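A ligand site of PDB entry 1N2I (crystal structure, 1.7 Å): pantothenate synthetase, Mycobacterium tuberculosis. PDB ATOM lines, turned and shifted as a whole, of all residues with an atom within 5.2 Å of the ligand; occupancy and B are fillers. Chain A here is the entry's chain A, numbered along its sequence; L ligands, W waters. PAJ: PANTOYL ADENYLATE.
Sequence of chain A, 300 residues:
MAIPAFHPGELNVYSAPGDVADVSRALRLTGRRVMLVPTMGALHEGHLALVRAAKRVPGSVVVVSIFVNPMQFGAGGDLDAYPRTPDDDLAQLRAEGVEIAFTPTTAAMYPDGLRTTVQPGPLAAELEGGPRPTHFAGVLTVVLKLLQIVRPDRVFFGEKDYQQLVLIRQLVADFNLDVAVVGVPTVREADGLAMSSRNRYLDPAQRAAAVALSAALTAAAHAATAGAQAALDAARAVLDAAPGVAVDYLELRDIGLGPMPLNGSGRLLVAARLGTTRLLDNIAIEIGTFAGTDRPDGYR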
ATOM      1  N   PRO A  38     -26.360 -15.642 -24.998  1.00  0.00           N
ATOM      2  CA  PRO A  38     -26.302 -14.414 -25.812  1.00  0.00           C
ATOM      3  C   PRO A  38     -25.142 -14.448 -26.781  1.00  0.00           C
ATOM      4  O   PRO A  38     -23.997 -14.753 -26.386  1.00  0.00           O
ATOM      5  CB  PRO A  38     -26.061 -13.305 -24.770  1.00  0.00           C
ATOM      6  CG  PRO A  38     -26.519 -13.953 -23.431  1.00  0.00           C
ATOM      7  CD  PRO A  38     -25.976 -15.346 -23.602  1.00  0.00           C
ATOM      8  N   THR A  39     -25.423 -14.115 -28.036  1.00  0.00           N
ATOM      9  CA  THR A  39     -24.361 -14.060 -29.038  1.00  0.00           C
ATOM     10  C   THR A  39     -24.660 -12.894 -29.972  1.00  0.00           C
ATOM     11  O   THR A  39     -25.757 -12.312 -29.945  1.00  0.00           O
ATOM     12  CB  THR A  39     -24.348 -15.297 -29.967  1.00  0.00           C
ATOM     13  OG1 THR A  39     -25.399 -15.170 -30.941  1.00  0.00           O
ATOM     14  CG2 THR A  39     -24.587 -16.610 -29.136  1.00  0.00           C
ATOM     15  N   MET A  40     -23.668 -12.575 -30.796  1.00  0.00           N
ATOM     16  CA  MET A  40     -23.850 -11.541 -31.819  1.00  0.00           C
ATOM     17  C   MET A  40     -23.778 -12.264 -33.165  1.00  0.00           C
ATOM     18  O   MET A  40     -23.430 -11.693 -34.207  1.00  0.00           O
ATOM     19  CB  MET A  40     -22.784 -10.450 -31.681  1.00  0.00           C
ATOM     20  CG  MET A  40     -22.855  -9.741 -30.330  1.00  0.00           C
ATOM     21  SD  MET A  40     -22.426  -7.966 -30.501  1.00  0.00           S
ATOM     22  CE  MET A  40     -20.770  -8.123 -30.886  1.00  0.00           C
ATOM     23  N   GLY A  41     -24.164 -13.540 -33.162  1.00  0.00           N
ATOM     24  CA  GLY A  41     -24.143 -14.302 -34.421  1.00  0.00           C
ATOM     25  C   GLY A  41     -22.765 -14.651 -34.961  1.00  0.00           C
ATOM     26  O   GLY A  41     -21.748 -14.590 -34.232  1.00  0.00           O
ATOM     27  N   HIS A  44     -19.634 -20.066 -34.443  1.00  0.00           N
ATOM     28  CA  HIS A  44     -18.584 -21.045 -34.682  1.00  0.00           C
ATOM     29  C   HIS A  44     -18.589 -22.041 -33.512  1.00  0.00           C
ATOM     30  O   HIS A  44     -19.467 -21.961 -32.640  1.00  0.00           O
ATOM     31  CB  HIS A  44     -17.219 -20.370 -34.813  1.00  0.00           C
ATOM     32  CG  HIS A  44     -16.866 -19.491 -33.653  1.00  0.00           C
ATOM     33  ND1 HIS A  44     -16.751 -19.964 -32.368  1.00  0.00           N
ATOM     34  CD2 HIS A  44     -16.625 -18.161 -33.594  1.00  0.00           C
ATOM     35  CE1 HIS A  44     -16.455 -18.954 -31.562  1.00  0.00           C
ATOM     36  NE2 HIS A  44     -16.377 -17.848 -32.280  1.00  0.00           N
ATOM     37  N   GLY A  46     -16.957 -22.267 -30.826  1.00  0.00           N
ATOM     38  CA  GLY A  46     -16.881 -21.706 -29.489  1.00  0.00           C
ATOM     39  C   GLY A  46     -18.298 -21.472 -28.991  1.00  0.00           C
ATOM     40  O   GLY A  46     -18.653 -21.824 -27.865  1.00  0.00           O
ATOM     41  N   HIS A  47     -19.127 -20.865 -29.836  1.00  0.00           N
ATOM     42  CA  HIS A  47     -20.522 -20.605 -29.454  1.00  0.00           C
ATOM     43  C   HIS A  47     -21.250 -21.896 -29.218  1.00  0.00           C
ATOM     44  O   HIS A  47     -22.088 -21.957 -28.324  1.00  0.00           O
ATOM     45  CB  HIS A  47     -21.274 -19.858 -30.545  1.00  0.00           C
ATOM     46  CG  HIS A  47     -20.692 -18.530 -30.888  1.00  0.00           C
ATOM     47  ND1 HIS A  47     -20.011 -18.299 -32.056  1.00  0.00           N
ATOM     48  CD2 HIS A  47     -20.670 -17.371 -30.195  1.00  0.00           C
ATOM     49  CE1 HIS A  47     -19.585 -17.040 -32.071  1.00  0.00           C
ATOM     50  NE2 HIS A  47     -19.980 -16.463 -30.958  1.00  0.00           N
ATOM     51  N   LEU A  50     -21.131 -23.334 -25.789  1.00  0.00           N
ATOM     52  CA  LEU A  50     -22.053 -22.687 -24.846  1.00  0.00           C
ATOM     53  C   LEU A  50     -23.443 -23.325 -25.024  1.00  0.00           C
ATOM     54  O   LEU A  50     -24.146 -23.660 -24.053  1.00  0.00           O
ATOM     55  CB  LEU A  50     -22.119 -21.170 -25.122  1.00  0.00           C
ATOM     56  CG  LEU A  50     -21.074 -20.311 -24.377  1.00  0.00           C
ATOM     57  CD1 LEU A  50     -19.676 -20.717 -24.786  1.00  0.00           C
ATOM     58  CD2 LEU A  50     -21.311 -18.829 -24.661  1.00  0.00           C
ATOM     59  N   PHE A  67     -27.902 -10.922 -31.830  1.00  0.00           N
ATOM     60  CA  PHE A  67     -28.179  -9.511 -31.974  1.00  0.00           C
ATOM     61  C   PHE A  67     -26.854  -8.771 -32.004  1.00  0.00           C
ATOM     62  O   PHE A  67     -26.077  -8.808 -31.037  1.00  0.00           O
ATOM     63  CB  PHE A  67     -29.059  -9.002 -30.797  1.00  0.00           C
ATOM     64  CG  PHE A  67     -29.322  -7.504 -30.827  1.00  0.00           C
ATOM     65  CD1 PHE A  67     -29.875  -6.898 -31.961  1.00  0.00           C
ATOM     66  CD2 PHE A  67     -29.059  -6.705 -29.710  1.00  0.00           C
ATOM     67  CE1 PHE A  67     -30.173  -5.513 -31.989  1.00  0.00           C
ATOM     68  CE2 PHE A  67     -29.342  -5.321 -29.722  1.00  0.00           C
ATOM     69  CZ  PHE A  67     -29.908  -4.725 -30.881  1.00  0.00           C
ATOM     70  N   ASN A  69     -25.368  -5.946 -31.262  1.00  0.00           N
ATOM     71  CA  ASN A  69     -25.699  -4.793 -30.416  1.00  0.00           C
ATOM     72  C   ASN A  69     -24.981  -3.503 -30.776  1.00  0.00           C
ATOM     73  O   ASN A  69     -23.800  -3.349 -30.472  1.00  0.00           O
ATOM     74  CB  ASN A  69     -25.354  -5.172 -28.986  1.00  0.00           C
ATOM     75  CG  ASN A  69     -25.606  -4.063 -28.021  1.00  0.00           C
ATOM     76  OD1 ASN A  69     -26.532  -3.242 -28.229  1.00  0.00           O
ATOM     77  ND2 ASN A  69     -24.808  -4.004 -26.960  1.00  0.00           N
ATOM     78  N   GLN A  72     -22.540  -1.341 -28.144  1.00  0.00           N
ATOM     79  CA  GLN A  72     -21.192  -1.721 -27.713  1.00  0.00           C
ATOM     80  C   GLN A  72     -20.124  -1.454 -28.754  1.00  0.00           C
ATOM     81  O   GLN A  72     -18.953  -1.830 -28.580  1.00  0.00           O
ATOM     82  CB  GLN A  72     -21.164  -3.175 -27.242  1.00  0.00           C
ATOM     83  CG  GLN A  72     -21.347  -4.257 -28.299  1.00  0.00           C
ATOM     84  CD  GLN A  72     -21.570  -5.615 -27.613  1.00  0.00           C
ATOM     85  OE1 GLN A  72     -22.600  -5.822 -26.991  1.00  0.00           O
ATOM     86  NE2 GLN A  72     -20.589  -6.503 -27.700  1.00  0.00           N
ATOM     87  N   TYR A  82     -18.891  -5.790 -38.702  1.00  0.00           N
ATOM     88  CA  TYR A  82     -19.048  -7.037 -37.949  1.00  0.00           C
ATOM     89  C   TYR A  82     -19.599  -8.125 -38.871  1.00  0.00           C
ATOM     90  O   TYR A  82     -20.551  -7.894 -39.616  1.00  0.00           O
ATOM     91  CB  TYR A  82     -19.995  -6.820 -36.778  1.00  0.00           C
ATOM     92  CG  TYR A  82     -19.784  -7.883 -35.736  1.00  0.00           C
ATOM     93  CD1 TYR A  82     -18.698  -7.823 -34.852  1.00  0.00           C
ATOM     94  CD2 TYR A  82     -20.638  -8.995 -35.673  1.00  0.00           C
ATOM     95  CE1 TYR A  82     -18.468  -8.835 -33.921  1.00  0.00           C
ATOM     96  CE2 TYR A  82     -20.417 -10.027 -34.754  1.00  0.00           C
ATOM     97  CZ  TYR A  82     -19.326  -9.935 -33.885  1.00  0.00           C
ATOM     98  OH  TYR A  82     -19.079 -10.943 -32.987  1.00  0.00           O
ATOM     99  N   VAL A 139     -22.398  -3.450 -23.567  1.00  0.00           N
ATOM    100  CA  VAL A 139     -22.538  -4.884 -23.304  1.00  0.00           C
ATOM    101  C   VAL A 139     -23.467  -5.114 -22.098  1.00  0.00           C
ATOM    102  O   VAL A 139     -24.397  -5.906 -22.183  1.00  0.00           O
ATOM    103  CB  VAL A 139     -21.137  -5.547 -22.977  1.00  0.00           C
ATOM    104  CG1 VAL A 139     -21.325  -7.034 -22.565  1.00  0.00           C
ATOM    105  CG2 VAL A 139     -20.175  -5.436 -24.201  1.00  0.00           C
ATOM    106  N   VAL A 142     -27.219  -4.205 -22.819  1.00  0.00           N
ATOM    107  CA  VAL A 142     -27.963  -5.163 -23.650  1.00  0.00           C
ATOM    108  C   VAL A 142     -28.159  -6.487 -22.895  1.00  0.00           C
ATOM    109  O   VAL A 142     -29.212  -7.132 -23.013  1.00  0.00           O
ATOM    110  CB  VAL A 142     -27.292  -5.389 -25.036  1.00  0.00           C
ATOM    111  CG1 VAL A 142     -26.128  -6.430 -24.988  1.00  0.00           C
ATOM    112  CG2 VAL A 142     -28.390  -5.833 -26.059  1.00  0.00           C
ATOM    113  N   VAL A 143     -27.165  -6.899 -22.113  1.00  0.00           N
ATOM    114  CA  VAL A 143     -27.310  -8.175 -21.379  1.00  0.00           C
ATOM    115  C   VAL A 143     -28.405  -8.059 -20.320  1.00  0.00           C
ATOM    116  O   VAL A 143     -29.172  -9.019 -20.101  1.00  0.00           O
ATOM    117  CB  VAL A 143     -25.969  -8.625 -20.752  1.00  0.00           C
ATOM    118  CG1 VAL A 143     -26.219  -9.823 -19.749  1.00  0.00           C
ATOM    119  CG2 VAL A 143     -24.989  -9.060 -21.865  1.00  0.00           C
ATOM    120  N   PHE A 156     -25.201 -18.273 -20.173  1.00  0.00           N
ATOM    121  CA  PHE A 156     -23.883 -18.796 -20.521  1.00  0.00           C
ATOM    122  C   PHE A 156     -22.988 -17.810 -21.262  1.00  0.00           C
ATOM    123  O   PHE A 156     -23.423 -17.188 -22.224  1.00  0.00           O
ATOM    124  CB  PHE A 156     -24.075 -20.063 -21.361  1.00  0.00           C
ATOM    125  CG  PHE A 156     -24.794 -21.172 -20.611  1.00  0.00           C
ATOM    126  CD1 PHE A 156     -26.169 -21.088 -20.382  1.00  0.00           C
ATOM    127  CD2 PHE A 156     -24.080 -22.220 -20.068  1.00  0.00           C
ATOM    128  CE1 PHE A 156     -26.824 -22.048 -19.580  1.00  0.00           C
ATOM    129  CE2 PHE A 156     -24.719 -23.205 -19.276  1.00  0.00           C
ATOM    130  CZ  PHE A 156     -26.093 -23.094 -19.035  1.00  0.00           C
ATOM    131  N   PHE A 157     -21.750 -17.708 -20.800  1.00  0.00           N
ATOM    132  CA  PHE A 157     -20.758 -16.819 -21.386  1.00  0.00           C
ATOM    133  C   PHE A 157     -19.419 -17.566 -21.527  1.00  0.00           C
ATOM    134  O   PHE A 157     -19.066 -18.406 -20.676  1.00  0.00           O
ATOM    135  CB  PHE A 157     -20.554 -15.600 -20.474  1.00  0.00           C
ATOM    136  CG  PHE A 157     -21.634 -14.587 -20.588  1.00  0.00           C
ATOM    137  CD1 PHE A 157     -22.725 -14.605 -19.750  1.00  0.00           C
ATOM    138  CD2 PHE A 157     -21.594 -13.635 -21.616  1.00  0.00           C
ATOM    139  CE1 PHE A 157     -23.760 -13.725 -19.905  1.00  0.00           C
ATOM    140  CE2 PHE A 157     -22.658 -12.726 -21.791  1.00  0.00           C
ATOM    141  CZ  PHE A 157     -23.738 -12.774 -20.935  1.00  0.00           C
ATOM    142  N   GLY A 158     -18.652 -17.250 -22.558  1.00  0.00           N
ATOM    143  CA  GLY A 158     -17.389 -17.930 -22.711  1.00  0.00           C
ATOM    144  C   GLY A 158     -16.243 -17.293 -21.928  1.00  0.00           C
ATOM    145  O   GLY A 158     -16.231 -16.086 -21.721  1.00  0.00           O
ATOM    146  N   GLU A 159     -15.273 -18.086 -21.505  1.00  0.00           N
ATOM    147  CA  GLU A 159     -14.112 -17.511 -20.812  1.00  0.00           C
ATOM    148  C   GLU A 159     -13.227 -16.738 -21.783  1.00  0.00           C
ATOM    149  O   GLU A 159     -12.371 -16.006 -21.379  1.00  0.00           O
ATOM    150  CB  GLU A 159     -13.295 -18.594 -20.152  1.00  0.00           C
ATOM    151  CG  GLU A 159     -14.086 -19.315 -19.070  1.00  0.00           C
ATOM    152  CD  GLU A 159     -13.216 -20.262 -18.254  1.00  0.00           C
ATOM    153  OE1 GLU A 159     -12.050 -20.476 -18.624  1.00  0.00           O
ATOM    154  OE2 GLU A 159     -13.719 -20.796 -17.256  1.00  0.00           O
ATOM    155  N   LYS A 160     -13.425 -16.937 -23.084  1.00  0.00           N
ATOM    156  CA  LYS A 160     -12.663 -16.232 -24.122  1.00  0.00           C
ATOM    157  C   LYS A 160     -12.686 -14.721 -23.862  1.00  0.00           C
ATOM    158  O   LYS A 160     -11.650 -14.055 -23.910  1.00  0.00           O
ATOM    159  CB  LYS A 160     -13.320 -16.535 -25.499  1.00  0.00           C
ATOM    160  CG  LYS A 160     -12.824 -15.661 -26.638  1.00  0.00           C
ATOM    161  CD  LYS A 160     -11.653 -16.312 -27.336  1.00  0.00           C
ATOM    162  CE  LYS A 160     -11.298 -15.571 -28.614  1.00  0.00           C
ATOM    163  NZ  LYS A 160     -11.119 -14.135 -28.318  1.00  0.00           N
ATOM    164  N   ASP A 161     -13.870 -14.194 -23.581  1.00  0.00           N
ATOM    165  CA  ASP A 161     -14.009 -12.764 -23.281  1.00  0.00           C
ATOM    166  C   ASP A 161     -14.133 -12.736 -21.767  1.00  0.00           C
ATOM    167  O   ASP A 161     -15.184 -12.469 -21.226  1.00  0.00           O
ATOM    168  CB  ASP A 161     -15.275 -12.242 -23.949  1.00  0.00           C
ATOM    169  CG  ASP A 161     -15.187 -12.330 -25.457  1.00  0.00           C
ATOM    170  OD1 ASP A 161     -14.500 -11.477 -26.021  1.00  0.00           O
ATOM    171  OD2 ASP A 161     -15.765 -13.258 -26.062  1.00  0.00           O
ATOM    172  N   GLN A 164     -15.355  -9.524 -19.955  1.00  0.00           N
ATOM    173  CA  GLN A 164     -16.795  -9.421 -20.138  1.00  0.00           C
ATOM    174  C   GLN A 164     -17.517 -10.332 -19.133  1.00  0.00           C
ATOM    175  O   GLN A 164     -18.479  -9.919 -18.516  1.00  0.00           O
ATOM    176  CB  GLN A 164     -17.171  -9.872 -21.548  1.00  0.00           C
ATOM    177  CG  GLN A 164     -18.666 -10.065 -21.707  1.00  0.00           C
ATOM    178  CD  GLN A 164     -19.049 -10.249 -23.147  1.00  0.00           C
ATOM    179  OE1 GLN A 164     -19.284  -9.268 -23.875  1.00  0.00           O
ATOM    180  NE2 GLN A 164     -19.043 -11.505 -23.616  1.00  0.00           N
ATOM    181  N   VAL A 184     -18.020 -20.812 -19.566  1.00  0.00           N
ATOM    182  CA  VAL A 184     -17.663 -21.999 -20.364  1.00  0.00           C
ATOM    183  C   VAL A 184     -16.239 -21.831 -20.879  1.00  0.00           C
ATOM    184  O   VAL A 184     -15.894 -20.789 -21.455  1.00  0.00           O
ATOM    185  CB  VAL A 184     -18.644 -22.149 -21.547  1.00  0.00           C
ATOM    186  CG1 VAL A 184     -18.332 -23.416 -22.374  1.00  0.00           C
ATOM    187  CG2 VAL A 184     -20.070 -22.211 -21.012  1.00  0.00           C
ATOM    188  N   PRO A 185     -15.385 -22.865 -20.707  1.00  0.00           N
ATOM    189  CA  PRO A 185     -13.988 -22.835 -21.143  1.00  0.00           C
ATOM    190  C   PRO A 185     -13.853 -22.528 -22.628  1.00  0.00           C
ATOM    191  O   PRO A 185     -14.673 -22.931 -23.473  1.00  0.00           O
ATOM    192  CB  PRO A 185     -13.474 -24.244 -20.799  1.00  0.00           C
ATOM    193  CG  PRO A 185     -14.333 -24.601 -19.578  1.00  0.00           C
ATOM    194  CD  PRO A 185     -15.694 -24.151 -20.041  1.00  0.00           C
ATOM    195  N   THR A 186     -12.796 -21.800 -22.923  1.00  0.00           N
ATOM    196  CA  THR A 186     -12.488 -21.411 -24.288  1.00  0.00           C
ATOM    197  C   THR A 186     -12.237 -22.590 -25.238  1.00  0.00           C
ATOM    198  O   THR A 186     -11.454 -23.492 -24.963  1.00  0.00           O
ATOM    199  CB  THR A 186     -11.259 -20.502 -24.278  1.00  0.00           C
ATOM    200  OG1 THR A 186     -11.606 -19.301 -23.585  1.00  0.00           O
ATOM    201  CG2 THR A 186     -10.783 -20.187 -25.684  1.00  0.00           C
ATOM    202  N   VAL A 187     -12.933 -22.564 -26.370  1.00  0.00           N
ATOM    203  CA  VAL A 187     -12.768 -23.601 -27.392  1.00  0.00           C
ATOM    204  C   VAL A 187     -11.639 -23.151 -28.310  1.00  0.00           C
ATOM    205  O   VAL A 187     -11.611 -21.985 -28.755  1.00  0.00           O
ATOM    206  CB  VAL A 187     -14.066 -23.805 -28.209  1.00  0.00           C
ATOM    207  CG1 VAL A 187     -13.830 -24.913 -29.227  1.00  0.00           C
ATOM    208  CG2 VAL A 187     -15.210 -24.161 -27.297  1.00  0.00           C
ATOM    209  N   ALA A 194      -7.467 -19.526 -30.024  1.00  0.00           N
ATOM    210  CA  ALA A 194      -8.814 -19.409 -29.444  1.00  0.00           C
ATOM    211  C   ALA A 194      -9.789 -19.136 -30.583  1.00  0.00           C
ATOM    212  O   ALA A 194      -9.521 -18.257 -31.412  1.00  0.00           O
ATOM    213  CB  ALA A 194      -8.876 -18.263 -28.445  1.00  0.00           C
ATOM    214  N   MET A 195     -10.886 -19.865 -30.658  1.00  0.00           N
ATOM    215  CA  MET A 195     -11.848 -19.583 -31.735  1.00  0.00           C
ATOM    216  C   MET A 195     -12.516 -18.222 -31.573  1.00  0.00           C
ATOM    217  O   MET A 195     -12.876 -17.803 -30.463  1.00  0.00           O
ATOM    218  CB  MET A 195     -12.889 -20.694 -31.830  1.00  0.00           C
ATOM    219  CG  MET A 195     -12.353 -21.909 -32.586  1.00  0.00           C
ATOM    220  SD  MET A 195     -13.624 -23.143 -32.780  1.00  0.00           S
ATOM    221  CE  MET A 195     -12.633 -24.636 -33.038  1.00  0.00           C
ATOM    222  N   SER A 196     -12.653 -17.521 -32.688  1.00  0.00           N
ATOM    223  CA  SER A 196     -13.251 -16.195 -32.712  1.00  0.00           C
ATOM    224  C   SER A 196     -13.814 -15.896 -34.086  1.00  0.00           C
ATOM    225  O   SER A 196     -13.271 -16.385 -35.082  1.00  0.00           O
ATOM    226  CB  SER A 196     -12.180 -15.149 -32.429  1.00  0.00           C
ATOM    227  OG  SER A 196     -12.687 -13.850 -32.641  1.00  0.00           O
ATOM    228  N   SER A 197     -14.882 -15.120 -34.148  1.00  0.00           N
ATOM    229  CA  SER A 197     -15.480 -14.751 -35.427  1.00  0.00           C
ATOM    230  C   SER A 197     -14.504 -13.853 -36.174  1.00  0.00           C
ATOM    231  O   SER A 197     -14.653 -13.620 -37.371  1.00  0.00           O
ATOM    232  CB  SER A 197     -16.800 -13.991 -35.194  1.00  0.00           C
ATOM    233  OG  SER A 197     -16.582 -12.820 -34.412  1.00  0.00           O
HETATM  234  P   PAJ L   1     -20.124 -13.002 -29.287  1.00  0.00           P
HETATM  235  O1P PAJ L   1     -18.848 -12.560 -29.838  1.00  0.00           O
HETATM  236  O2P PAJ L   1     -21.165 -13.489 -30.274  1.00  0.00           O
HETATM  237  O5' PAJ L   1     -19.769 -14.180 -28.188  1.00  0.00           O
HETATM  238  C5' PAJ L   1     -20.848 -14.638 -27.751  1.00  0.00           C
HETATM  239  C4' PAJ L   1     -20.434 -15.552 -26.535  1.00  0.00           C
HETATM  240  O4' PAJ L   1     -19.678 -16.735 -26.964  1.00  0.00           O
HETATM  241  C3' PAJ L   1     -19.533 -14.857 -25.478  1.00  0.00           C
HETATM  242  O3' PAJ L   1     -19.960 -15.296 -24.212  1.00  0.00           O
HETATM  243  C2' PAJ L   1     -18.178 -15.333 -25.827  1.00  0.00           C
HETATM  244  O2' PAJ L   1     -17.162 -15.181 -24.827  1.00  0.00           O
HETATM  245  C1' PAJ L   1     -18.437 -16.780 -26.245  1.00  0.00           C
HETATM  246  N9  PAJ L   1     -17.316 -17.226 -27.058  1.00  0.00           N
HETATM  247  C8  PAJ L   1     -16.752 -16.682 -28.219  1.00  0.00           C
HETATM  248  N7  PAJ L   1     -15.744 -17.302 -28.732  1.00  0.00           N
HETATM  249  C5  PAJ L   1     -15.599 -18.389 -27.848  1.00  0.00           C
HETATM  250  C6  PAJ L   1     -14.684 -19.496 -27.782  1.00  0.00           C
HETATM  251  N6  PAJ L   1     -13.709 -19.676 -28.674  1.00  0.00           N
HETATM  252  N1  PAJ L   1     -14.843 -20.438 -26.711  1.00  0.00           N
HETATM  253  C2  PAJ L   1     -15.829 -20.298 -25.763  1.00  0.00           C
HETATM  254  N3  PAJ L   1     -16.751 -19.257 -25.740  1.00  0.00           N
HETATM  255  C4  PAJ L   1     -16.581 -18.346 -26.816  1.00  0.00           C
HETATM  256  O11 PAJ L   1     -19.825 -11.380 -26.361  1.00  0.00           O
HETATM  257  C11 PAJ L   1     -20.726 -10.974 -27.211  1.00  0.00           C
HETATM  258  O12 PAJ L   1     -20.807 -11.756 -28.553  1.00  0.00           O
HETATM  259  C12 PAJ L   1     -21.599  -9.746 -26.848  1.00  0.00           C
HETATM  260  O13 PAJ L   1     -20.792  -8.809 -26.064  1.00  0.00           O
HETATM  261  C13 PAJ L   1     -22.945 -10.144 -26.045  1.00  0.00           C
HETATM  262  C14 PAJ L   1     -23.829 -11.124 -26.834  1.00  0.00           C
HETATM  263  C15 PAJ L   1     -22.596 -10.722 -24.645  1.00  0.00           C
HETATM  264  C16 PAJ L   1     -23.661  -8.817 -25.845  1.00  0.00           C
HETATM  265  O14 PAJ L   1     -23.939  -8.223 -27.109  1.00  0.00           O
HETATM  266  O   HOH W   1     -22.677 -15.407 -24.253  1.00  0.00           O
HETATM  267  O   HOH W   2     -26.360  -8.745 -28.232  1.00  0.00           O
HETATM  268  O   HOH W   3     -20.115 -13.194 -33.005  1.00  0.00           O
HETATM  269  O   HOH W   4     -16.673 -14.462 -31.473  1.00  0.00           O
HETATM  270  O   HOH W   5     -17.824 -13.641 -21.870  1.00  0.00           O
HETATM  271  O   HOH W   6     -16.394 -13.275 -28.638  1.00  0.00           O
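Water W1 lies within hydrogen-bond range of O of Pro 38 (2.6 Å), O3' of the ligand (2.7 Å) and O of Phe 156 (2.8 Å). Water W2 lies within hydrogen-bond range of an oxygen (O14) of the ligand and the backbone carbonyl oxygen of Phe 67. Water W6 lies within hydrogen-bond range of the side-chain carboxylate (OD2) of Asp 161 (2.7 Å) and an oxygen (O1P) of the ligand (2.8 Å). Water W3 lies within hydrogen-bond range of O of Gly 41, OH of Tyr 82 and O2P of the ligand. Water W4 lies within hydrogen-bond range of the backbone NH of Ser 197 (3.3 Å), an oxygen (O1P) of the ligand (3.3 Å) and a ring nitrogen (NE2) of His 44 (3.5 Å). Water W5 lies within hydrogen-bond range of the backbone carbonyl oxygen of Gly 158 (2.9 Å), the backbone carbonyl oxygen of Asp 161 (3.0 Å), the side-chain amide nitrogen of Gln 164 (3.0 Å) and an oxygen (O2') of the ligand (3.4 Å).
OD2 of Asp 161 sits at hydrogen-bond distance from O2' of the ligand (2.7 Å). The side-chain amide oxygen (OE1) of Gln 164 is in hydrogen-bond range of an oxygen (O13) of the ligand, at 2.7 Å. N of Met 40 is in hydrogen-bond range of O2P of the ligand, at 2.7 Å. An oxygen (O14) of the ligand lies close to the side-chain sulfur (SD) of Met 40, at 3.7 Å. The backbone carbonyl oxygen (O) of Met 195 sits at hydrogen-bond distance from a nitrogen (N6) of the ligand, at 2.7 Å. The side-chain amide oxygen of Gln 72 lies within hydrogen-bond range of an oxygen (O14) of the ligand, 2.8 Å away. An oxygen (O3') of the ligand sits at hydrogen-bond distance from the backbone NH (N) of Gly 158. The backbone carbonyl oxygen (O) of Gly 158 sits at hydrogen-bond distance from an oxygen (O2') of the ligand. N of Val 187 sits at hydrogen-bond distance from N1 of the ligand (2.9 Å). O of Val 187 sits at hydrogen-bond distance from N6 of the ligand. A ring nitrogen (NE2) of His 47 sits at hydrogen-bond distance from an oxygen (O2P) of the ligand.
Pro 38 touches the ligand (O to C5', 3.4 Å). Thr 39 touches the ligand (CA to O2P, 3.5 Å). His 44 touches the ligand (CE1 to N7, 3.4 Å). Gly 46 touches the ligand (CA to C6, 3.6 Å). CD1 of Leu 50 touches N3 of the ligand (3.4 Å). CB of Asn 69 touches O14 of the ligand (3.9 Å). Tyr 82 touches the ligand (OH to O1P, 3.5 Å). Val 139 touches the ligand (CG2 to O13, 3.9 Å). Val 142 touches the ligand (CG1 to O14, 3.5 Å). Phe 157 touches the ligand (CA to O3', 3.3 Å). CB of Lys 160 touches C5 of the ligand, 3.8 Å away. Pro 185 touches the ligand. CA of Thr 186 touches N1 of the ligand, at 3.5 Å. Hydrophobic or aromatic side chains within 4 Å of the ligand: Pro 38, Met 40, His 44, His 47, Leu 50, Val 139, Val 142, Phe 157, Val 187 and Met 195. Within 4 Å of the ligand: Pro 38, Thr 39, Met 40, His 44, Gly 46, His 47, Leu 50, Asn 69, Gln 72, Tyr 82, Val 139, Val 142, Phe 157, Gly 158, Lys 160, Asp 161, Gln 164, Pro 185, Thr 186, Val 187 and Met 195. The nearest printed residue that does not touch the ligand is Val 143 (4.03 Å).
The backbone NH (N) of Asn 69 lies within hydrogen-bond range of the side-chain sulfur (SD) of Met 40. The backbone NH of Met 195 is in hydrogen-bond range of the backbone carbonyl oxygen of Val 187 (2.9 Å). OE1 of Gln 72 sits at hydrogen-bond distance from ND2 of Asn 69, at 2.9 Å. ND1 of His 47 is in hydrogen-bond range of N of His 44 (3.0 Å). A ring nitrogen (ND1) of His 44 sits at hydrogen-bond distance from the backbone NH (N) of Gly 46, 2.8 Å away. N of Phe 67 is in hydrogen-bond range of O of Thr 39 (3.2 Å). OG1 of Thr 186 lies within hydrogen-bond range of N of Lys 160. The side-chain hydroxyl of Ser 197 lies within hydrogen-bond range of the side-chain hydroxyl of Tyr 82, at 3.4 Å.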
